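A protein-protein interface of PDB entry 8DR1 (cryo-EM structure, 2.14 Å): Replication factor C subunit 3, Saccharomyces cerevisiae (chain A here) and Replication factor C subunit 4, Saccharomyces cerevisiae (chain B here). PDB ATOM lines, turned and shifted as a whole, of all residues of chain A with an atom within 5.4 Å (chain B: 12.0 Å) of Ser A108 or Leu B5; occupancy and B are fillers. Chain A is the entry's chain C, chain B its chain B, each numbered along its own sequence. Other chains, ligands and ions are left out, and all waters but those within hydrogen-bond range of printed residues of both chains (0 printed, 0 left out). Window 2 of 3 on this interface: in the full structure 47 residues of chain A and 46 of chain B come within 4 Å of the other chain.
The side-chain hydroxyl of Tyr A71 is in hydrogen-bond range of the backbone carbonyl oxygen of Phe A111. The backbone carbonyl oxygen of Phe A111 lies within hydrogen-bond range of the side-chain amide nitrogen of Gln A105. The side-chain hydroxyl of Ser A108 lies within hydrogen-bond range of the backbone NH of Gly A110 (2.9 Å).
Thr B4 touches Ile A70. O of Ile A70 touches CD2 of Leu B5, 3.5 Å away. OG of Ser A108 touches CD1 of Leu B5, 3.8 Å away. Leu B5 touches Gly A110 (O to CA, 3.6 Å). Thr B4 touches Phe A111 (O to CE2, 3.8 Å). O of Leu B5 touches N of Phe A111, at 3.7 Å. Phe A111 touches Leu B7 (CB to CD1, 3.6 Å).
Of the printed residues of chain B, Ser A108 touches Leu B5. Leu B5 touches just these residues of chain A: Ile A70, Ser A108, Gly A110 and Phe A111. Of chain B, only Thr B4 (3.8 Å) and Leu B5 (3.5 Å) come within 4 Å of Ile A70. Gln A105 touches none of the printed residues of chain B. No residue of chain B comes within 4 Å of Phe A107. No residue of chain B comes within 4 Å of Lys A109. Gly A110 touches one residue of chain B. Phe A111 touches three residues of chain B. Of the printed residues of chain A, Leu B7 touches Phe A111 (3.6 Å). Of the printed residues of chain A, Thr B4 touches Ile A70 and Phe A111. The nearest residue of chain B that does not touch Ser A108 is Thr B4 (8.6 Å). The nearest residue of chain A that does not touch Leu B5 is Tyr A71 (4.03 Å). The nearest printed residue of chain A that does not touch Thr B4 is Tyr A71 (6.2 Å).
Of the 10 printed residues of chain A, 4 touch a printed residue of chain B. Hydrophobic or aromatic side chains of chain A that line the printed part of chain B: Ile A70 and Phe A111. Of the 6 printed residues of chain B, 3 touch a printed residue of chain A. Among the printed residues, no Asp or Glu carboxylate lies within 4 Å of a Lys or Arg side-chain nitrogen of the other chain.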
ATOM      1  N   ILE A  70       1.299  -3.502  -5.344  1.00  0.00           N
ATOM      2  CA  ILE A  70       2.723  -3.673  -5.070  1.00  0.00           C
ATOM      3  C   ILE A  70       3.557  -2.806  -6.006  1.00  0.00           C
ATOM      4  O   ILE A  70       4.477  -2.104  -5.571  1.00  0.00           O
ATOM      5  CB  ILE A  70       3.118  -5.157  -5.181  1.00  0.00           C
ATOM      6  CG1 ILE A  70       2.549  -5.953  -4.005  1.00  0.00           C
ATOM      7  CG2 ILE A  70       4.634  -5.305  -5.236  1.00  0.00           C
ATOM      8  CD1 ILE A  70       2.447  -7.440  -4.271  1.00  0.00           C
ATOM      9  N   TYR A  71       3.247  -2.836  -7.305  1.00  0.00           N
ATOM     10  CA  TYR A  71       4.094  -2.214  -8.313  1.00  0.00           C
ATOM     11  C   TYR A  71       3.530  -0.925  -8.891  1.00  0.00           C
ATOM     12  O   TYR A  71       4.308  -0.105  -9.390  1.00  0.00           O
ATOM     13  CB  TYR A  71       4.346  -3.194  -9.467  1.00  0.00           C
ATOM     14  CG  TYR A  71       5.046  -4.464  -9.041  1.00  0.00           C
ATOM     15  CD1 TYR A  71       6.408  -4.475  -8.773  1.00  0.00           C
ATOM     16  CD2 TYR A  71       4.341  -5.652  -8.900  1.00  0.00           C
ATOM     17  CE1 TYR A  71       7.050  -5.632  -8.382  1.00  0.00           C
ATOM     18  CE2 TYR A  71       4.974  -6.815  -8.508  1.00  0.00           C
ATOM     19  CZ  TYR A  71       6.327  -6.800  -8.250  1.00  0.00           C
ATOM     20  OH  TYR A  71       6.962  -7.956  -7.861  1.00  0.00           O
ATOM     21  N   MET A  78       6.259  -5.820 -14.815  1.00  0.00           N
ATOM     22  CA  MET A  78       7.006  -6.199 -13.625  1.00  0.00           C
ATOM     23  C   MET A  78       6.603  -7.557 -13.066  1.00  0.00           C
ATOM     24  O   MET A  78       7.147  -7.972 -12.038  1.00  0.00           O
ATOM     25  CB  MET A  78       6.830  -5.129 -12.542  1.00  0.00           C
ATOM     26  CG  MET A  78       7.419  -3.778 -12.915  1.00  0.00           C
ATOM     27  SD  MET A  78       7.590  -2.691 -11.492  1.00  0.00           S
ATOM     28  CE  MET A  78       9.269  -3.060 -10.995  1.00  0.00           C
ATOM     29  N   GLN A 105      14.746  -7.058 -11.684  1.00  0.00           N
ATOM     30  CA  GLN A 105      13.762  -6.306 -12.450  1.00  0.00           C
ATOM     31  C   GLN A 105      14.456  -5.296 -13.357  1.00  0.00           C
ATOM     32  O   GLN A 105      15.474  -4.704 -12.990  1.00  0.00           O
ATOM     33  CB  GLN A 105      12.795  -5.580 -11.514  1.00  0.00           C
ATOM     34  CG  GLN A 105      11.916  -6.496 -10.674  1.00  0.00           C
ATOM     35  CD  GLN A 105      10.539  -6.704 -11.277  1.00  0.00           C
ATOM     36  OE1 GLN A 105      10.339  -6.516 -12.476  1.00  0.00           O
ATOM     37  NE2 GLN A 105       9.582  -7.092 -10.443  1.00  0.00           N
ATOM     38  N   ILE A 106      13.900  -5.106 -14.554  1.00  0.00           N
ATOM     39  CA  ILE A 106      14.455  -4.119 -15.474  1.00  0.00           C
ATOM     40  C   ILE A 106      14.205  -2.707 -14.957  1.00  0.00           C
ATOM     41  O   ILE A 106      15.097  -1.850 -14.994  1.00  0.00           O
ATOM     42  CB  ILE A 106      13.870  -4.309 -16.886  1.00  0.00           C
ATOM     43  CG1 ILE A 106      14.098  -5.743 -17.372  1.00  0.00           C
ATOM     44  CG2 ILE A 106      14.489  -3.307 -17.858  1.00  0.00           C
ATOM     45  CD1 ILE A 106      13.554  -6.015 -18.758  1.00  0.00           C
ATOM     46  N   PHE A 107      12.998  -2.443 -14.459  1.00  0.00           N
ATOM     47  CA  PHE A 107      12.577  -1.080 -14.155  1.00  0.00           C
ATOM     48  C   PHE A 107      12.986  -0.635 -12.753  1.00  0.00           C
ATOM     49  O   PHE A 107      13.620   0.413 -12.597  1.00  0.00           O
ATOM     50  CB  PHE A 107      11.060  -0.962 -14.335  1.00  0.00           C
ATOM     51  CG  PHE A 107      10.603  -1.182 -15.749  1.00  0.00           C
ATOM     52  CD1 PHE A 107      10.324  -2.457 -16.210  1.00  0.00           C
ATOM     53  CD2 PHE A 107      10.466  -0.115 -16.622  1.00  0.00           C
ATOM     54  CE1 PHE A 107       9.909  -2.665 -17.511  1.00  0.00           C
ATOM     55  CE2 PHE A 107      10.052  -0.317 -17.925  1.00  0.00           C
ATOM     56  CZ  PHE A 107       9.773  -1.594 -18.370  1.00  0.00           C
ATOM     57  N   SER A 108      12.637  -1.408 -11.731  1.00  0.00           N
ATOM     58  CA  SER A 108      12.902  -1.050 -10.343  1.00  0.00           C
ATOM     59  C   SER A 108      13.815  -2.095  -9.702  1.00  0.00           C
ATOM     60  O   SER A 108      14.353  -2.981 -10.373  1.00  0.00           O
ATOM     61  CB  SER A 108      11.594  -0.908  -9.565  1.00  0.00           C
ATOM     62  OG  SER A 108      11.312  -2.089  -8.832  1.00  0.00           O
ATOM     63  N   LYS A 109      13.998  -1.971  -8.387  1.00  0.00           N
ATOM     64  CA  LYS A 109      14.815  -2.893  -7.610  1.00  0.00           C
ATOM     65  C   LYS A 109      13.980  -3.809  -6.723  1.00  0.00           C
ATOM     66  O   LYS A 109      14.540  -4.523  -5.884  1.00  0.00           O
ATOM     67  CB  LYS A 109      15.814  -2.111  -6.754  1.00  0.00           C
ATOM     68  CG  LYS A 109      16.751  -1.220  -7.556  1.00  0.00           C
ATOM     69  CD  LYS A 109      16.697   0.219  -7.071  1.00  0.00           C
ATOM     70  CE  LYS A 109      17.415   1.156  -8.026  1.00  0.00           C
ATOM     71  NZ  LYS A 109      16.464   1.904  -8.895  1.00  0.00           N
ATOM     72  N   GLY A 110      12.658  -3.810  -6.887  1.00  0.00           N
ATOM     73  CA  GLY A 110      11.788  -4.605  -6.049  1.00  0.00           C
ATOM     74  C   GLY A 110      11.824  -6.079  -6.399  1.00  0.00           C
ATOM     75  O   GLY A 110      12.452  -6.515  -7.363  1.00  0.00           O
ATOM     76  N   PHE A 111      11.124  -6.863  -5.583  1.00  0.00           N
ATOM     77  CA  PHE A 111      11.068  -8.299  -5.796  1.00  0.00           C
ATOM     78  C   PHE A 111      10.188  -8.620  -7.006  1.00  0.00           C
ATOM     79  O   PHE A 111       9.558  -7.745  -7.607  1.00  0.00           O
ATOM     80  CB  PHE A 111      10.562  -9.006  -4.537  1.00  0.00           C
ATOM     81  CG  PHE A 111       9.096  -8.808  -4.266  1.00  0.00           C
ATOM     82  CD1 PHE A 111       8.153  -9.666  -4.810  1.00  0.00           C
ATOM     83  CD2 PHE A 111       8.663  -7.771  -3.458  1.00  0.00           C
ATOM     84  CE1 PHE A 111       6.808  -9.487  -4.557  1.00  0.00           C
ATOM     85  CE2 PHE A 111       7.317  -7.589  -3.201  1.00  0.00           C
ATOM     86  CZ  PHE A 111       6.389  -8.448  -3.752  1.00  0.00           C
ATOM     87  N   THR B   4       4.957  -1.817  -1.125  1.00  0.00           N
ATOM     88  CA  THR B   4       6.212  -2.272  -0.540  1.00  0.00           C
ATOM     89  C   THR B   4       6.945  -3.195  -1.507  1.00  0.00           C
ATOM     90  O   THR B   4       6.346  -4.096  -2.095  1.00  0.00           O
ATOM     91  CB  THR B   4       5.979  -3.008   0.792  1.00  0.00           C
ATOM     92  OG1 THR B   4       5.395  -2.110   1.743  1.00  0.00           O
ATOM     93  CG2 THR B   4       7.289  -3.551   1.346  1.00  0.00           C
ATOM     94  N   LEU B   5       8.248  -2.962  -1.665  1.00  0.00           N
ATOM     95  CA  LEU B   5       9.078  -3.711  -2.601  1.00  0.00           C
ATOM     96  C   LEU B   5      10.149  -4.533  -1.892  1.00  0.00           C
ATOM     97  O   LEU B   5      11.178  -4.854  -2.494  1.00  0.00           O
ATOM     98  CB  LEU B   5       9.722  -2.755  -3.606  1.00  0.00           C
ATOM     99  CG  LEU B   5       8.780  -2.044  -4.583  1.00  0.00           C
ATOM    100  CD1 LEU B   5       9.579  -1.224  -5.582  1.00  0.00           C
ATOM    101  CD2 LEU B   5       7.872  -3.030  -5.307  1.00  0.00           C
ATOM    102  N   SER B   6       9.926  -4.883  -0.629  1.00  0.00           N
ATOM    103  CA  SER B   6      10.868  -5.660   0.160  1.00  0.00           C
ATOM    104  C   SER B   6      10.228  -6.971   0.598  1.00  0.00           C
ATOM    105  O   SER B   6       9.007  -7.079   0.733  1.00  0.00           O
ATOM    106  CB  SER B   6      11.339  -4.871   1.386  1.00  0.00           C
ATOM    107  OG  SER B   6      10.239  -4.366   2.121  1.00  0.00           O
ATOM    108  N   LEU B   7      11.077  -7.974   0.818  1.00  0.00           N
ATOM    109  CA  LEU B   7      10.639  -9.311   1.187  1.00  0.00           C
ATOM    110  C   LEU B   7      11.360  -9.765   2.446  1.00  0.00           C
ATOM    111  O   LEU B   7      12.573  -9.582   2.580  1.00  0.00           O
ATOM    112  CB  LEU B   7      10.906 -10.314   0.053  1.00  0.00           C
ATOM    113  CG  LEU B   7       9.916 -10.372  -1.113  1.00  0.00           C
ATOM    114  CD1 LEU B   7      10.284 -11.522  -2.040  1.00  0.00           C
ATOM    115  CD2 LEU B   7       8.478 -10.516  -0.631  1.00  0.00           C
ATOM    116  N   GLN B   8      10.606 -10.365   3.363  1.00  0.00           N
ATOM    117  CA  GLN B   8      11.171 -10.989   4.551  1.00  0.00           C
ATOM    118  C   GLN B   8      11.503 -12.441   4.232  1.00  0.00           C
ATOM    119  O   GLN B   8      10.648 -13.183   3.740  1.00  0.00           O
ATOM    120  CB  GLN B   8      10.190 -10.894   5.724  1.00  0.00           C
ATOM    121  CG  GLN B   8      10.522 -11.770   6.929  1.00  0.00           C
ATOM    122  CD  GLN B   8       9.374 -11.855   7.915  1.00  0.00           C
ATOM    123  OE1 GLN B   8       8.551 -12.767   7.850  1.00  0.00           O
ATOM    124  NE2 GLN B   8       9.316 -10.904   8.838  1.00  0.00           N
ATOM    125  N   LEU B   9      12.737 -12.839   4.508  1.00  0.00           N
ATOM    126  CA  LEU B   9      13.176 -14.183   4.165  1.00  0.00           C
ATOM    127  C   LEU B   9      12.313 -15.210   4.898  1.00  0.00           C
ATOM    128  O   LEU B   9      12.118 -15.091   6.115  1.00  0.00           O
ATOM    129  CB  LEU B   9      14.648 -14.375   4.528  1.00  0.00           C
ATOM    130  CG  LEU B   9      15.290 -15.676   4.039  1.00  0.00           C
ATOM    131  CD1 LEU B   9      15.498 -15.638   2.534  1.00  0.00           C
ATOM    132  CD2 LEU B   9      16.612 -15.925   4.751  1.00  0.00           C
